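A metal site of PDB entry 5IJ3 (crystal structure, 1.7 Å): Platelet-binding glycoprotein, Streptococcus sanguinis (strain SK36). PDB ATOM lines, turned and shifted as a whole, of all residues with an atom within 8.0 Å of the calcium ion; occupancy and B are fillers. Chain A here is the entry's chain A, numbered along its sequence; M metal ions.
The calcium ion is bound by OD1 of Asp 31 (2.4 Å), O of Thr 4 (2.4 Å), OD2 of Asp 102 (2.4 Å), OD2 of Asp 30 (2.4 Å), OD1 of Asp 30 (2.4 Å), OD2 of Asp 2 (2.4 Å) and OD1 of Asp 2 (2.4 Å). The calcium ion has seven donor atoms within binding distance.
Five residues have an atom within 4 Å of the calcium ion: Asp 2, Thr 4, Asp 30, Asp 31 and Asp 102. The nearest printed residue that does not touch the calcium ion is Asn 106 (4.2 Å).
The side-chain amide nitrogen of Asn 106 sits at hydrogen-bond distance from the backbone carbonyl oxygen of Asp 2 (2.9 Å). The backbone NH (N) of Asn 106 lies within hydrogen-bond range of the side-chain carboxylate (OD1) of Asp 102 (2.9 Å). The side-chain hydroxyl (OG) of Ser 32 lies close to the side-chain carboxylate (OD2) of Asp 30 (2.6 Å). The side-chain carboxylate (OD1) of Asp 102 lies within hydrogen-bond range of the backbone NH (N) of Gly 105, at 3.2 Å. The side-chain carboxylate (OD1) of Asp 102 lies within hydrogen-bond range of the backbone NH (N) of Ala 104, at 2.8 Å.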
ATOM      1  N   THR A   1     -36.568 -26.663 -12.519  1.00  0.00           N
ATOM      2  CA  THR A   1     -35.796 -25.710 -13.298  1.00  0.00           C
ATOM      3  C   THR A   1     -34.314 -26.073 -13.347  1.00  0.00           C
ATOM      4  O   THR A   1     -33.812 -26.832 -12.518  1.00  0.00           O
ATOM      5  CB  THR A   1     -35.928 -24.273 -12.750  1.00  0.00           C
ATOM      6  OG1 THR A   1     -35.639 -24.283 -11.342  1.00  0.00           O
ATOM      7  CG2 THR A   1     -37.324 -23.748 -12.976  1.00  0.00           C
ATOM      8  N   ASP A   2     -33.634 -25.519 -14.348  1.00  0.00           N
ATOM      9  CA  ASP A   2     -32.185 -25.598 -14.469  1.00  0.00           C
ATOM     10  C   ASP A   2     -31.565 -24.499 -13.607  1.00  0.00           C
ATOM     11  O   ASP A   2     -31.756 -23.317 -13.864  1.00  0.00           O
ATOM     12  CB  ASP A   2     -31.780 -25.438 -15.940  1.00  0.00           C
ATOM     13  CG  ASP A   2     -30.272 -25.632 -16.187  1.00  0.00           C
ATOM     14  OD1 ASP A   2     -29.454 -25.554 -15.241  1.00  0.00           O
ATOM     15  OD2 ASP A   2     -29.886 -25.855 -17.347  1.00  0.00           O
ATOM     16  N   THR A   3     -30.837 -24.905 -12.567  1.00  0.00           N
ATOM     17  CA  THR A   3     -30.184 -23.939 -11.682  1.00  0.00           C
ATOM     18  C   THR A   3     -28.678 -24.163 -11.632  1.00  0.00           C
ATOM     19  O   THR A   3     -27.987 -23.567 -10.795  1.00  0.00           O
ATOM     20  CB  THR A   3     -30.737 -24.023 -10.250  1.00  0.00           C
ATOM     21  OG1 THR A   3     -30.505 -25.339  -9.738  1.00  0.00           O
ATOM     22  CG2 THR A   3     -32.242 -23.735 -10.227  1.00  0.00           C
ATOM     23  N   THR A   4     -28.185 -25.023 -12.505  1.00  0.00           N
ATOM     24  CA  THR A   4     -26.783 -25.421 -12.496  1.00  0.00           C
ATOM     25  C   THR A   4     -26.029 -24.826 -13.688  1.00  0.00           C
ATOM     26  O   THR A   4     -26.423 -25.039 -14.814  1.00  0.00           O
ATOM     27  CB  THR A   4     -26.652 -26.953 -12.530  1.00  0.00           C
ATOM     28  OG1 THR A   4     -27.423 -27.518 -11.461  1.00  0.00           O
ATOM     29  CG2 THR A   4     -25.196 -27.374 -12.393  1.00  0.00           C
ATOM     30  N   PRO A   5     -24.949 -24.068 -13.445  1.00  0.00           N
ATOM     31  CA  PRO A   5     -24.253 -23.492 -14.596  1.00  0.00           C
ATOM     32  C   PRO A   5     -23.424 -24.534 -15.370  1.00  0.00           C
ATOM     33  O   PRO A   5     -23.227 -25.647 -14.867  1.00  0.00           O
ATOM     34  CB  PRO A   5     -23.344 -22.444 -13.954  1.00  0.00           C
ATOM     35  CG  PRO A   5     -23.051 -22.989 -12.614  1.00  0.00           C
ATOM     36  CD  PRO A   5     -24.293 -23.721 -12.168  1.00  0.00           C
ATOM     37  N   PRO A   6     -22.959 -24.165 -16.568  1.00  0.00           N
ATOM     38  CA  PRO A   6     -22.097 -25.048 -17.349  1.00  0.00           C
ATOM     39  C   PRO A   6     -20.780 -25.377 -16.646  1.00  0.00           C
ATOM     40  O   PRO A   6     -20.356 -24.670 -15.739  1.00  0.00           O
ATOM     41  CB  PRO A   6     -21.820 -24.236 -18.625  1.00  0.00           C
ATOM     42  CG  PRO A   6     -22.970 -23.316 -18.730  1.00  0.00           C
ATOM     43  CD  PRO A   6     -23.316 -22.953 -17.318  1.00  0.00           C
ATOM     44  N   THR A   7     -20.149 -26.455 -17.093  1.00  0.00           N
ATOM     45  CA  THR A   7     -18.852 -26.867 -16.588  1.00  0.00           C
ATOM     46  C   THR A   7     -17.801 -26.765 -17.677  1.00  0.00           C
ATOM     47  O   THR A   7     -17.959 -27.330 -18.753  1.00  0.00           O
ATOM     48  CB  THR A   7     -18.888 -28.320 -16.074  1.00  0.00           C
ATOM     49  OG1 THR A   7     -19.851 -28.434 -15.020  1.00  0.00           O
ATOM     50  CG2 THR A   7     -17.527 -28.741 -15.575  1.00  0.00           C
ATOM     51  N   THR A  29     -19.635 -28.429 -21.006  1.00  0.00           N
ATOM     52  CA  THR A  29     -20.885 -29.190 -20.929  1.00  0.00           C
ATOM     53  C   THR A  29     -21.877 -28.457 -20.028  1.00  0.00           C
ATOM     54  O   THR A  29     -21.486 -27.632 -19.213  1.00  0.00           O
ATOM     55  CB  THR A  29     -20.664 -30.611 -20.372  1.00  0.00           C
ATOM     56  OG1 THR A  29     -20.307 -30.531 -18.984  1.00  0.00           O
ATOM     57  CG2 THR A  29     -19.560 -31.336 -21.130  1.00  0.00           C
ATOM     58  N   ASP A  30     -23.173 -28.745 -20.188  1.00  0.00           N
ATOM     59  CA  ASP A  30     -24.184 -28.269 -19.243  1.00  0.00           C
ATOM     60  C   ASP A  30     -25.215 -29.358 -19.050  1.00  0.00           C
ATOM     61  O   ASP A  30     -25.466 -30.150 -19.974  1.00  0.00           O
ATOM     62  CB  ASP A  30     -24.869 -26.986 -19.740  1.00  0.00           C
ATOM     63  CG  ASP A  30     -25.869 -26.422 -18.707  1.00  0.00           C
ATOM     64  OD1 ASP A  30     -25.430 -25.866 -17.687  1.00  0.00           O
ATOM     65  OD2 ASP A  30     -27.095 -26.529 -18.907  1.00  0.00           O
ATOM     66  N   ASP A  31     -25.816 -29.411 -17.871  1.00  0.00           N
ATOM     67  CA  ASP A  31     -26.795 -30.470 -17.604  1.00  0.00           C
ATOM     68  C   ASP A  31     -27.999 -30.400 -18.554  1.00  0.00           C
ATOM     69  O   ASP A  31     -28.635 -31.420 -18.811  1.00  0.00           O
ATOM     70  CB  ASP A  31     -27.259 -30.428 -16.128  1.00  0.00           C
ATOM     71  CG  ASP A  31     -27.899 -29.102 -15.715  1.00  0.00           C
ATOM     72  OD1 ASP A  31     -27.540 -28.047 -16.256  1.00  0.00           O
ATOM     73  OD2 ASP A  31     -28.766 -29.121 -14.812  1.00  0.00           O
ATOM     74  N   SER A  32     -28.270 -29.220 -19.108  1.00  0.00           N
ATOM     75  CA  SER A  32     -29.354 -29.045 -20.075  1.00  0.00           C
ATOM     76  C   SER A  32     -28.962 -29.493 -21.467  1.00  0.00           C
ATOM     77  O   SER A  32     -29.818 -29.657 -22.343  1.00  0.00           O
ATOM     78  CB  SER A  32     -29.784 -27.581 -20.156  1.00  0.00           C
ATOM     79  OG  SER A  32     -28.811 -26.818 -20.856  1.00  0.00           O
ATOM     80  N   GLY A  33     -27.655 -29.635 -21.690  1.00  0.00           N
ATOM     81  CA  GLY A  33     -27.125 -29.940 -22.998  1.00  0.00           C
ATOM     82  C   GLY A  33     -26.957 -28.742 -23.919  1.00  0.00           C
ATOM     83  O   GLY A  33     -26.575 -28.904 -25.071  1.00  0.00           O
ATOM     84  N   GLN A  34     -27.229 -27.536 -23.420  1.00  0.00           N
ATOM     85  CA  GLN A  34     -27.112 -26.332 -24.248  1.00  0.00           C
ATOM     86  C   GLN A  34     -26.308 -25.237 -23.559  1.00  0.00           C
ATOM     87  O   GLN A  34     -26.647 -24.815 -22.451  1.00  0.00           O
ATOM     88  CB  GLN A  34     -28.495 -25.789 -24.616  1.00  0.00           C
ATOM     89  CG  GLN A  34     -28.450 -24.600 -25.563  1.00  0.00           C
ATOM     90  CD  GLN A  34     -29.824 -24.206 -26.071  1.00  0.00           C
ATOM     91  OE1 GLN A  34     -30.785 -24.954 -25.925  1.00  0.00           O
ATOM     92  NE2 GLN A  34     -29.932 -23.022 -26.670  1.00  0.00           N
ATOM     93  N   VAL A  35     -25.260 -24.772 -24.229  1.00  0.00           N
ATOM     94  CA  VAL A  35     -24.490 -23.614 -23.771  1.00  0.00           C
ATOM     95  C   VAL A  35     -24.756 -22.439 -24.701  1.00  0.00           C
ATOM     96  O   VAL A  35     -24.675 -22.569 -25.925  1.00  0.00           O
ATOM     97  CB  VAL A  35     -22.986 -23.929 -23.701  1.00  0.00           C
ATOM     98  CG1 VAL A  35     -22.156 -22.645 -23.634  1.00  0.00           C
ATOM     99  CG2 VAL A  35     -22.693 -24.801 -22.484  1.00  0.00           C
ATOM    100  N   TRP A 101     -22.429 -19.278 -20.033  1.00  0.00           N
ATOM    101  CA  TRP A 101     -23.863 -19.259 -19.710  1.00  0.00           C
ATOM    102  C   TRP A 101     -24.564 -20.448 -20.328  1.00  0.00           C
ATOM    103  O   TRP A 101     -24.218 -20.857 -21.439  1.00  0.00           O
ATOM    104  CB  TRP A 101     -24.539 -17.993 -20.262  1.00  0.00           C
ATOM    105  CG  TRP A 101     -24.309 -16.691 -19.532  1.00  0.00           C
ATOM    106  CD1 TRP A 101     -25.168 -16.060 -18.673  1.00  0.00           C
ATOM    107  CD2 TRP A 101     -23.157 -15.839 -19.643  1.00  0.00           C
ATOM    108  NE1 TRP A 101     -24.614 -14.889 -18.218  1.00  0.00           N
ATOM    109  CE2 TRP A 101     -23.378 -14.726 -18.791  1.00  0.00           C
ATOM    110  CE3 TRP A 101     -21.955 -15.916 -20.351  1.00  0.00           C
ATOM    111  CZ2 TRP A 101     -22.449 -13.703 -18.651  1.00  0.00           C
ATOM    112  CZ3 TRP A 101     -21.023 -14.885 -20.205  1.00  0.00           C
ATOM    113  CH2 TRP A 101     -21.281 -13.803 -19.361  1.00  0.00           C
ATOM    114  N   ASP A 102     -25.547 -21.006 -19.637  1.00  0.00           N
ATOM    115  CA  ASP A 102     -26.477 -21.920 -20.309  1.00  0.00           C
ATOM    116  C   ASP A 102     -27.670 -21.112 -20.830  1.00  0.00           C
ATOM    117  O   ASP A 102     -27.635 -19.883 -20.794  1.00  0.00           O
ATOM    118  CB  ASP A 102     -26.913 -23.070 -19.392  1.00  0.00           C
ATOM    119  CG  ASP A 102     -27.687 -22.616 -18.153  1.00  0.00           C
ATOM    120  OD1 ASP A 102     -28.215 -21.486 -18.108  1.00  0.00           O
ATOM    121  OD2 ASP A 102     -27.775 -23.436 -17.208  1.00  0.00           O
ATOM    122  N   ALA A 103     -28.696 -21.791 -21.323  1.00  0.00           N
ATOM    123  CA  ALA A 103     -29.848 -21.098 -21.905  1.00  0.00           C
ATOM    124  C   ALA A 103     -30.872 -20.673 -20.862  1.00  0.00           C
ATOM    125  O   ALA A 103     -31.908 -20.099 -21.200  1.00  0.00           O
ATOM    126  CB  ALA A 103     -30.511 -21.982 -22.953  1.00  0.00           C
ATOM    127  N   ALA A 104     -30.585 -20.948 -19.590  1.00  0.00           N
ATOM    128  CA  ALA A 104     -31.525 -20.663 -18.509  1.00  0.00           C
ATOM    129  C   ALA A 104     -31.028 -19.532 -17.603  1.00  0.00           C
ATOM    130  O   ALA A 104     -31.595 -19.286 -16.535  1.00  0.00           O
ATOM    131  CB  ALA A 104     -31.779 -21.918 -17.677  1.00  0.00           C
ATOM    132  N   GLY A 105     -29.966 -18.864 -18.021  1.00  0.00           N
ATOM    133  CA  GLY A 105     -29.450 -17.733 -17.289  1.00  0.00           C
ATOM    134  C   GLY A 105     -28.388 -18.052 -16.254  1.00  0.00           C
ATOM    135  O   GLY A 105     -27.892 -17.157 -15.578  1.00  0.00           O
ATOM    136  N   ASN A 106     -28.042 -19.330 -16.113  1.00  0.00           N
ATOM    137  CA  ASN A 106     -26.986 -19.710 -15.188  1.00  0.00           C
ATOM    138  C   ASN A 106     -25.613 -19.481 -15.805  1.00  0.00           C
ATOM    139  O   ASN A 106     -25.320 -19.994 -16.886  1.00  0.00           O
ATOM    140  CB  ASN A 106     -27.128 -21.171 -14.767  1.00  0.00           C
ATOM    141  CG  ASN A 106     -28.497 -21.467 -14.185  1.00  0.00           C
ATOM    142  OD1 ASN A 106     -28.858 -20.942 -13.136  1.00  0.00           O
ATOM    143  ND2 ASN A 106     -29.258 -22.331 -14.861  1.00  0.00           N
ATOM    144  N   VAL A 107     -24.770 -18.722 -15.120  1.00  0.00           N
ATOM    145  CA  VAL A 107     -23.415 -18.475 -15.589  1.00  0.00           C
ATOM    146  C   VAL A 107     -22.419 -19.107 -14.622  1.00  0.00           C
ATOM    147  O   VAL A 107     -22.589 -19.045 -13.397  1.00  0.00           O
ATOM    148  CB  VAL A 107     -23.137 -16.957 -15.770  1.00  0.00           C
ATOM    149  CG1 VAL A 107     -23.338 -16.204 -14.460  1.00  0.00           C
ATOM    150  CG2 VAL A 107     -21.751 -16.718 -16.353  1.00  0.00           C
HETATM  151 CA    CA M   1     -27.597 -25.743 -16.728  1.00  0.00          CA
